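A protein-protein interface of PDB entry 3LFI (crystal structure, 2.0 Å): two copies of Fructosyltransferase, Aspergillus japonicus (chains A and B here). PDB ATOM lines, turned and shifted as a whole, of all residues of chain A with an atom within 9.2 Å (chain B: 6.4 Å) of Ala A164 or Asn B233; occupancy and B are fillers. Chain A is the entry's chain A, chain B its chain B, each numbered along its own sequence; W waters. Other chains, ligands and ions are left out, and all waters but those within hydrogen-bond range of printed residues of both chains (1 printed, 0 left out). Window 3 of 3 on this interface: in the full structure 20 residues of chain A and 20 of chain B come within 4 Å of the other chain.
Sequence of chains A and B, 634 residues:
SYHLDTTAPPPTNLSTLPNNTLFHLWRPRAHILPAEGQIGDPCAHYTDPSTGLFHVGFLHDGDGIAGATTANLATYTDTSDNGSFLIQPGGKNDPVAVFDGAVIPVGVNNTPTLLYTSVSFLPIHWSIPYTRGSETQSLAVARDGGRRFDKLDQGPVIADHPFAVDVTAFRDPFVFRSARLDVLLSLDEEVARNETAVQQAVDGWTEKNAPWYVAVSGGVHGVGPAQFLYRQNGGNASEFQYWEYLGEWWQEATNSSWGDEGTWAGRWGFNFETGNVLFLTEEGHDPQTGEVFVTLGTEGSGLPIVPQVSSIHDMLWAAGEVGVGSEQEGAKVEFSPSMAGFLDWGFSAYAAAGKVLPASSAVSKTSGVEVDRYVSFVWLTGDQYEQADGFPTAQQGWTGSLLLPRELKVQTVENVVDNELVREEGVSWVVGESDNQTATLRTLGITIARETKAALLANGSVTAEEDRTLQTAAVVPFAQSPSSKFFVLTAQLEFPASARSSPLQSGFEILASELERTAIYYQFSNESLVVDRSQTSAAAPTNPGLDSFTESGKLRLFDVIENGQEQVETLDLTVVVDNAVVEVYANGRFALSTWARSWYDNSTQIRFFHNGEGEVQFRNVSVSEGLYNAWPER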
ATOM      1  N   ARG A 132      28.973  -1.209 -15.443  1.00  0.00           N
ATOM      2  CA  ARG A 132      29.773   0.017 -15.466  1.00  0.00           C
ATOM      3  C   ARG A 132      30.780  -0.046 -16.618  1.00  0.00           C
ATOM      4  O   ARG A 132      31.403  -1.084 -16.844  1.00  0.00           O
ATOM      5  CB  ARG A 132      30.514   0.186 -14.122  1.00  0.00           C
ATOM      6  CG  ARG A 132      31.312   1.504 -13.953  1.00  0.00           C
ATOM      7  CD  ARG A 132      30.399   2.721 -13.717  1.00  0.00           C
ATOM      8  NE  ARG A 132      31.139   3.942 -13.383  1.00  0.00           N
ATOM      9  CZ  ARG A 132      31.809   4.140 -12.248  1.00  0.00           C
ATOM     10  NH1 ARG A 132      31.847   3.204 -11.309  1.00  0.00           N
ATOM     11  NH2 ARG A 132      32.451   5.282 -12.046  1.00  0.00           N
ATOM     12  N   ASP A 160      32.468   8.134 -18.821  1.00  0.00           N
ATOM     13  CA  ASP A 160      31.539   7.525 -17.878  1.00  0.00           C
ATOM     14  C   ASP A 160      30.227   8.296 -17.878  1.00  0.00           C
ATOM     15  O   ASP A 160      30.190   9.460 -18.254  1.00  0.00           O
ATOM     16  CB  ASP A 160      32.186   7.520 -16.484  1.00  0.00           C
ATOM     17  CG  ASP A 160      31.366   6.763 -15.442  1.00  0.00           C
ATOM     18  OD1 ASP A 160      30.705   5.759 -15.777  1.00  0.00           O
ATOM     19  OD2 ASP A 160      31.408   7.175 -14.264  1.00  0.00           O
ATOM     20  N   HIS A 161      29.143   7.634 -17.486  1.00  0.00           N
ATOM     21  CA  HIS A 161      27.845   8.295 -17.426  1.00  0.00           C
ATOM     22  C   HIS A 161      27.883   9.190 -16.185  1.00  0.00           C
ATOM     23  O   HIS A 161      28.823   9.107 -15.392  1.00  0.00           O
ATOM     24  CB  HIS A 161      26.732   7.257 -17.290  1.00  0.00           C
ATOM     25  CG  HIS A 161      26.885   6.362 -16.098  1.00  0.00           C
ATOM     26  ND1 HIS A 161      26.871   6.836 -14.803  1.00  0.00           N
ATOM     27  CD2 HIS A 161      27.063   5.023 -16.007  1.00  0.00           C
ATOM     28  CE1 HIS A 161      27.033   5.828 -13.966  1.00  0.00           C
ATOM     29  NE2 HIS A 161      27.153   4.717 -14.670  1.00  0.00           N
ATOM     30  N   PRO A 162      26.878  10.065 -16.008  1.00  0.00           N
ATOM     31  CA  PRO A 162      26.861  10.948 -14.834  1.00  0.00           C
ATOM     32  C   PRO A 162      27.165  10.209 -13.520  1.00  0.00           C
ATOM     33  O   PRO A 162      26.629   9.127 -13.263  1.00  0.00           O
ATOM     34  CB  PRO A 162      25.458  11.531 -14.883  1.00  0.00           C
ATOM     35  CG  PRO A 162      25.279  11.723 -16.380  1.00  0.00           C
ATOM     36  CD  PRO A 162      25.789  10.407 -16.940  1.00  0.00           C
ATOM     37  N   PHE A 163      28.015  10.818 -12.697  1.00  0.00           N
ATOM     38  CA  PHE A 163      28.458  10.238 -11.431  1.00  0.00           C
ATOM     39  C   PHE A 163      27.387   9.658 -10.529  1.00  0.00           C
ATOM     40  O   PHE A 163      26.437  10.344 -10.145  1.00  0.00           O
ATOM     41  CB  PHE A 163      29.265  11.259 -10.624  1.00  0.00           C
ATOM     42  CG  PHE A 163      29.812  10.711  -9.330  1.00  0.00           C
ATOM     43  CD1 PHE A 163      30.859   9.790  -9.335  1.00  0.00           C
ATOM     44  CD2 PHE A 163      29.259  11.094  -8.105  1.00  0.00           C
ATOM     45  CE1 PHE A 163      31.352   9.253  -8.134  1.00  0.00           C
ATOM     46  CE2 PHE A 163      29.739  10.566  -6.902  1.00  0.00           C
ATOM     47  CZ  PHE A 163      30.789   9.643  -6.916  1.00  0.00           C
ATOM     48  N   ALA A 164      27.573   8.384 -10.187  1.00  0.00           N
ATOM     49  CA  ALA A 164      26.679   7.644  -9.303  1.00  0.00           C
ATOM     50  C   ALA A 164      25.232   7.579  -9.769  1.00  0.00           C
ATOM     51  O   ALA A 164      24.332   7.347  -8.966  1.00  0.00           O
ATOM     52  CB  ALA A 164      26.742   8.231  -7.896  1.00  0.00           C
ATOM     53  N   VAL A 165      24.998   7.790 -11.058  1.00  0.00           N
ATOM     54  CA  VAL A 165      23.640   7.716 -11.582  1.00  0.00           C
ATOM     55  C   VAL A 165      23.473   6.353 -12.229  1.00  0.00           C
ATOM     56  O   VAL A 165      24.219   6.003 -13.143  1.00  0.00           O
ATOM     57  CB  VAL A 165      23.377   8.824 -12.611  1.00  0.00           C
ATOM     58  CG1 VAL A 165      21.987   8.666 -13.197  1.00  0.00           C
ATOM     59  CG2 VAL A 165      23.519  10.184 -11.938  1.00  0.00           C
ATOM     60  N   ASP A 166      22.497   5.585 -11.745  1.00  0.00           N
ATOM     61  CA  ASP A 166      22.245   4.233 -12.245  1.00  0.00           C
ATOM     62  C   ASP A 166      21.489   4.245 -13.575  1.00  0.00           C
ATOM     63  O   ASP A 166      20.304   3.897 -13.647  1.00  0.00           O
ATOM     64  CB  ASP A 166      21.467   3.436 -11.188  1.00  0.00           C
ATOM     65  CG  ASP A 166      21.413   1.942 -11.497  1.00  0.00           C
ATOM     66  OD1 ASP A 166      22.173   1.480 -12.373  1.00  0.00           O
ATOM     67  OD2 ASP A 166      20.614   1.223 -10.855  1.00  0.00           O
ATOM     68  N   VAL A 167      22.189   4.635 -14.634  1.00  0.00           N
ATOM     69  CA  VAL A 167      21.578   4.713 -15.959  1.00  0.00           C
ATOM     70  C   VAL A 167      21.126   3.375 -16.523  1.00  0.00           C
ATOM     71  O   VAL A 167      21.700   2.325 -16.230  1.00  0.00           O
ATOM     72  CB  VAL A 167      22.541   5.355 -16.993  1.00  0.00           C
ATOM     73  CG1 VAL A 167      22.934   6.758 -16.548  1.00  0.00           C
ATOM     74  CG2 VAL A 167      23.765   4.475 -17.178  1.00  0.00           C
ATOM     75  N   VAL A 220      17.235   6.371 -16.253  1.00  0.00           N
ATOM     76  CA  VAL A 220      17.723   6.078 -14.913  1.00  0.00           C
ATOM     77  C   VAL A 220      16.838   5.003 -14.273  1.00  0.00           C
ATOM     78  O   VAL A 220      15.609   5.152 -14.179  1.00  0.00           O
ATOM     79  CB  VAL A 220      17.720   7.366 -14.044  1.00  0.00           C
ATOM     80  CG1 VAL A 220      18.291   7.082 -12.667  1.00  0.00           C
ATOM     81  CG2 VAL A 220      18.550   8.458 -14.738  1.00  0.00           C
ATOM     82  N   HIS A 221      17.465   3.906 -13.856  1.00  0.00           N
ATOM     83  CA  HIS A 221      16.748   2.806 -13.237  1.00  0.00           C
ATOM     84  C   HIS A 221      15.831   3.290 -12.121  1.00  0.00           C
ATOM     85  O   HIS A 221      16.228   4.108 -11.284  1.00  0.00           O
ATOM     86  CB  HIS A 221      17.733   1.782 -12.671  1.00  0.00           C
ATOM     87  CG  HIS A 221      18.294   0.845 -13.694  1.00  0.00           C
ATOM     88  ND1 HIS A 221      17.594  -0.240 -14.177  1.00  0.00           N
ATOM     89  CD2 HIS A 221      19.484   0.845 -14.342  1.00  0.00           C
ATOM     90  CE1 HIS A 221      18.329  -0.869 -15.078  1.00  0.00           C
ATOM     91  NE2 HIS A 221      19.481  -0.230 -15.198  1.00  0.00           N
ATOM     92  N   TYR A 245      29.007  18.433 -18.253  1.00  0.00           N
ATOM     93  CA  TYR A 245      27.685  17.840 -18.123  1.00  0.00           C
ATOM     94  C   TYR A 245      26.710  18.922 -17.678  1.00  0.00           C
ATOM     95  O   TYR A 245      26.928  19.593 -16.668  1.00  0.00           O
ATOM     96  CB  TYR A 245      27.726  16.693 -17.104  1.00  0.00           C
ATOM     97  CG  TYR A 245      26.387  16.023 -16.861  1.00  0.00           C
ATOM     98  CD1 TYR A 245      25.557  15.678 -17.925  1.00  0.00           C
ATOM     99  CD2 TYR A 245      25.962  15.717 -15.565  1.00  0.00           C
ATOM    100  CE1 TYR A 245      24.334  15.045 -17.716  1.00  0.00           C
ATOM    101  CE2 TYR A 245      24.739  15.082 -15.342  1.00  0.00           C
ATOM    102  CZ  TYR A 245      23.932  14.750 -16.426  1.00  0.00           C
ATOM    103  OH  TYR A 245      22.725  14.133 -16.219  1.00  0.00           O
ATOM    104  N   GLU A 248      20.339  16.256 -16.864  1.00  0.00           N
ATOM    105  CA  GLU A 248      19.285  15.560 -17.594  1.00  0.00           C
ATOM    106  C   GLU A 248      18.256  16.604 -18.016  1.00  0.00           C
ATOM    107  O   GLU A 248      17.208  16.756 -17.393  1.00  0.00           O
ATOM    108  CB  GLU A 248      18.645  14.502 -16.689  1.00  0.00           C
ATOM    109  CG  GLU A 248      19.600  13.377 -16.323  1.00  0.00           C
ATOM    110  CD  GLU A 248      19.018  12.403 -15.316  1.00  0.00           C
ATOM    111  OE1 GLU A 248      17.803  12.127 -15.395  1.00  0.00           O
ATOM    112  OE2 GLU A 248      19.779  11.900 -14.458  1.00  0.00           O
ATOM    113  N   ARG B 231      36.909   8.878  -1.799  1.00  0.00           N
ATOM    114  CA  ARG B 231      36.384   8.032  -0.736  1.00  0.00           C
ATOM    115  C   ARG B 231      35.049   7.462  -1.190  1.00  0.00           C
ATOM    116  O   ARG B 231      34.360   8.060  -2.021  1.00  0.00           O
ATOM    117  CB  ARG B 231      36.227   8.809   0.585  1.00  0.00           C
ATOM    118  CG  ARG B 231      34.986   9.678   0.717  1.00  0.00           C
ATOM    119  CD  ARG B 231      34.709   9.979   2.206  1.00  0.00           C
ATOM    120  NE  ARG B 231      33.382  10.551   2.428  1.00  0.00           N
ATOM    121  CZ  ARG B 231      32.869  10.828   3.627  1.00  0.00           C
ATOM    122  NH1 ARG B 231      33.566  10.590   4.733  1.00  0.00           N
ATOM    123  NH2 ARG B 231      31.652  11.348   3.720  1.00  0.00           N
ATOM    124  N   GLN B 232      34.704   6.288  -0.675  1.00  0.00           N
ATOM    125  CA  GLN B 232      33.447   5.652  -1.027  1.00  0.00           C
ATOM    126  C   GLN B 232      32.348   6.712  -1.028  1.00  0.00           C
ATOM    127  O   GLN B 232      32.179   7.446  -0.053  1.00  0.00           O
ATOM    128  CB  GLN B 232      33.138   4.550  -0.023  1.00  0.00           C
ATOM    129  CG  GLN B 232      34.155   3.427  -0.065  1.00  0.00           C
ATOM    130  CD  GLN B 232      33.886   2.362   0.966  1.00  0.00           C
ATOM    131  OE1 GLN B 232      34.045   2.588   2.167  1.00  0.00           O
ATOM    132  NE2 GLN B 232      33.473   1.190   0.505  1.00  0.00           N
ATOM    133  N   ASN B 233      31.610   6.793  -2.127  1.00  0.00           N
ATOM    134  CA  ASN B 233      30.561   7.793  -2.263  1.00  0.00           C
ATOM    135  C   ASN B 233      29.683   7.939  -1.021  1.00  0.00           C
ATOM    136  O   ASN B 233      29.235   6.954  -0.436  1.00  0.00           O
ATOM    137  CB  ASN B 233      29.704   7.482  -3.489  1.00  0.00           C
ATOM    138  CG  ASN B 233      28.806   8.640  -3.878  1.00  0.00           C
ATOM    139  OD1 ASN B 233      29.202   9.801  -3.786  1.00  0.00           O
ATOM    140  ND2 ASN B 233      27.598   8.331  -4.326  1.00  0.00           N
ATOM    141  N   GLY B 234      29.462   9.188  -0.622  1.00  0.00           N
ATOM    142  CA  GLY B 234      28.645   9.480   0.543  1.00  0.00           C
ATOM    143  C   GLY B 234      29.130   8.853   1.839  1.00  0.00           C
ATOM    144  O   GLY B 234      28.360   8.733   2.797  1.00  0.00           O
ATOM    145  N   GLY B 235      30.401   8.457   1.881  1.00  0.00           N
ATOM    146  CA  GLY B 235      30.946   7.840   3.077  1.00  0.00           C
ATOM    147  C   GLY B 235      30.318   6.488   3.362  1.00  0.00           C
ATOM    148  O   GLY B 235      30.290   6.026   4.504  1.00  0.00           O
ATOM    149  N   ASN B 236      29.818   5.841   2.317  1.00  0.00           N
ATOM    150  CA  ASN B 236      29.173   4.540   2.453  1.00  0.00           C
ATOM    151  C   ASN B 236      30.206   3.419   2.390  1.00  0.00           C
ATOM    152  O   ASN B 236      30.674   3.070   1.310  1.00  0.00           O
ATOM    153  CB  ASN B 236      28.152   4.354   1.327  1.00  0.00           C
ATOM    154  CG  ASN B 236      27.196   3.209   1.583  1.00  0.00           C
ATOM    155  OD1 ASN B 236      27.529   2.243   2.264  1.00  0.00           O
ATOM    156  ND2 ASN B 236      25.998   3.308   1.020  1.00  0.00           N
ATOM    157  N   ALA B 237      30.552   2.855   3.544  1.00  0.00           N
ATOM    158  CA  ALA B 237      31.535   1.775   3.615  1.00  0.00           C
ATOM    159  C   ALA B 237      31.175   0.585   2.729  1.00  0.00           C
ATOM    160  O   ALA B 237      32.022  -0.259   2.433  1.00  0.00           O
ATOM    161  CB  ALA B 237      31.701   1.312   5.063  1.00  0.00           C
ATOM    162  N   GLU B 239      29.924   0.967  -0.346  1.00  0.00           N
ATOM    163  CA  GLU B 239      29.945   1.427  -1.731  1.00  0.00           C
ATOM    164  C   GLU B 239      31.309   1.229  -2.392  1.00  0.00           C
ATOM    165  O   GLU B 239      32.235   1.985  -2.124  1.00  0.00           O
ATOM    166  CB  GLU B 239      29.567   2.908  -1.784  1.00  0.00           C
ATOM    167  CG  GLU B 239      29.635   3.514  -3.174  1.00  0.00           C
ATOM    168  CD  GLU B 239      28.741   2.789  -4.160  1.00  0.00           C
ATOM    169  OE1 GLU B 239      27.511   3.008  -4.127  1.00  0.00           O
ATOM    170  OE2 GLU B 239      29.272   1.989  -4.960  1.00  0.00           O
ATOM    171  N   TYR B 242      31.144   3.551  -6.713  1.00  0.00           N
ATOM    172  CA  TYR B 242      31.362   4.985  -6.874  1.00  0.00           C
ATOM    173  C   TYR B 242      32.222   5.615  -5.782  1.00  0.00           C
ATOM    174  O   TYR B 242      32.002   5.398  -4.588  1.00  0.00           O
ATOM    175  CB  TYR B 242      30.005   5.682  -6.960  1.00  0.00           C
ATOM    176  CG  TYR B 242      29.185   5.179  -8.125  1.00  0.00           C
ATOM    177  CD1 TYR B 242      29.517   5.531  -9.433  1.00  0.00           C
ATOM    178  CD2 TYR B 242      28.108   4.308  -7.928  1.00  0.00           C
ATOM    179  CE1 TYR B 242      28.804   5.028 -10.519  1.00  0.00           C
ATOM    180  CE2 TYR B 242      27.382   3.798  -9.008  1.00  0.00           C
ATOM    181  CZ  TYR B 242      27.739   4.166 -10.303  1.00  0.00           C
ATOM    182  OH  TYR B 242      27.031   3.687 -11.388  1.00  0.00           O
ATOM    183  N   TRP B 243      33.204   6.399  -6.211  1.00  0.00           N
ATOM    184  CA  TRP B 243      34.120   7.061  -5.294  1.00  0.00           C
ATOM    185  C   TRP B 243      34.068   8.560  -5.510  1.00  0.00           C
ATOM    186  O   TRP B 243      34.518   9.053  -6.540  1.00  0.00           O
ATOM    187  CB  TRP B 243      35.540   6.544  -5.526  1.00  0.00           C
ATOM    188  CG  TRP B 243      35.600   5.055  -5.462  1.00  0.00           C
ATOM    189  CD1 TRP B 243      35.102   4.172  -6.381  1.00  0.00           C
ATOM    190  CD2 TRP B 243      36.078   4.270  -4.371  1.00  0.00           C
ATOM    191  NE1 TRP B 243      35.236   2.882  -5.921  1.00  0.00           N
ATOM    192  CE2 TRP B 243      35.833   2.915  -4.689  1.00  0.00           C
ATOM    193  CE3 TRP B 243      36.688   4.580  -3.145  1.00  0.00           C
ATOM    194  CZ2 TRP B 243      36.180   1.869  -3.826  1.00  0.00           C
ATOM    195  CZ3 TRP B 243      37.031   3.541  -2.290  1.00  0.00           C
ATOM    196  CH2 TRP B 243      36.776   2.203  -2.636  1.00  0.00           C
ATOM    197  N   GLU B 244      33.521   9.289  -4.542  1.00  0.00           N
ATOM    198  CA  GLU B 244      33.428  10.737  -4.680  1.00  0.00           C
ATOM    199  C   GLU B 244      34.807  11.386  -4.612  1.00  0.00           C
ATOM    200  O   GLU B 244      35.639  11.010  -3.794  1.00  0.00           O
ATOM    201  CB  GLU B 244      32.530  11.332  -3.588  1.00  0.00           C
ATOM    202  CG  GLU B 244      32.966  11.016  -2.168  1.00  0.00           C
ATOM    203  CD  GLU B 244      32.131  11.740  -1.112  1.00  0.00           C
ATOM    204  OE1 GLU B 244      32.303  11.440   0.090  1.00  0.00           O
ATOM    205  OE2 GLU B 244      31.313  12.612  -1.483  1.00  0.00           O
HETATM  206  O   HOH W   1      26.675   1.966 -13.865  1.00  0.00           O
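NE2 of His A161 sits close to OH of Tyr B242, 3.4 Å away.
The backbone NH (N) of Asn B233 is in hydrogen-bond range of the backbone carbonyl oxygen (O) of Tyr B242 (2.9 Å).
A ring nitrogen (ND1) of His A161 sits close to the backbone carbonyl oxygen (O) of Val A165, 3.2 Å away.
NE of Arg B231 lies within salt-bridge range of OE1 of Glu B244 (2.7 Å).
The side-chain carboxylate (OD1) of Asp A160 lies within salt-bridge range of the guanidinium group (NE) of Arg A132 (3.0 Å).
OE2 of Glu B239 sits at hydrogen-bond distance from N of Tyr B242, 3.0 Å away.
Among the printed residues, pairs that only touch across the chains: Phe A163 with Asn B233 (3.3 Å), Ala A164 with Tyr B242 (3.5 Å), Phe A163 with Trp B243 (3.6 Å), Arg A132 with Tyr B242 (3.6 Å), Phe A163 with Glu B244 (3.6 Å), Ala A164 with Asn B233 (3.7 Å) and Phe A163 with Tyr B242 (3.99 Å).
Of the printed residues of chain B, Ala A164 touches Asn B233 and Tyr B242.
Of chain A, only Phe A163 (3.3 Å) and Ala A164 (3.7 Å) come within 4 Å of Asn B233.
No residue of chain A comes within 4 Å of Gly B234.
No residue of chain A comes within 4 Å of Gly B235.
Of the printed residues of chain A, Glu B244 touches Phe A163 (3.6 Å).
Of the printed residues of chain B, Arg A132 touches Tyr B242 (3.6 Å).
Printed residues of chain B that touch a printed residue of chain A: Asn B233, Tyr B242, Trp B243 and Glu B244.
Hydrophobic or aromatic side chains of chain B within 4 Å of the printed part of chain A: Tyr B242.
Hydrophobic or aromatic side chains of chain A that line the printed part of chain B: His A161, Phe A163 and Ala A164.
Along chain A the printed residues that touch a printed residue of chain B span positions 132 to 164.
Among the printed residues, 8 pairs touch across the chains.
Among the printed residues, no Asp or Glu carboxylate lies within 4 Å of a Lys or Arg side-chain nitrogen of the other chain.
No position is printed for both chains.
Water W1 lies within hydrogen-bond range of a ring nitrogen (NE2) of His A161 (2.9 Å) and the side-chain hydroxyl (OH) of Tyr B242 (3.0 Å).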
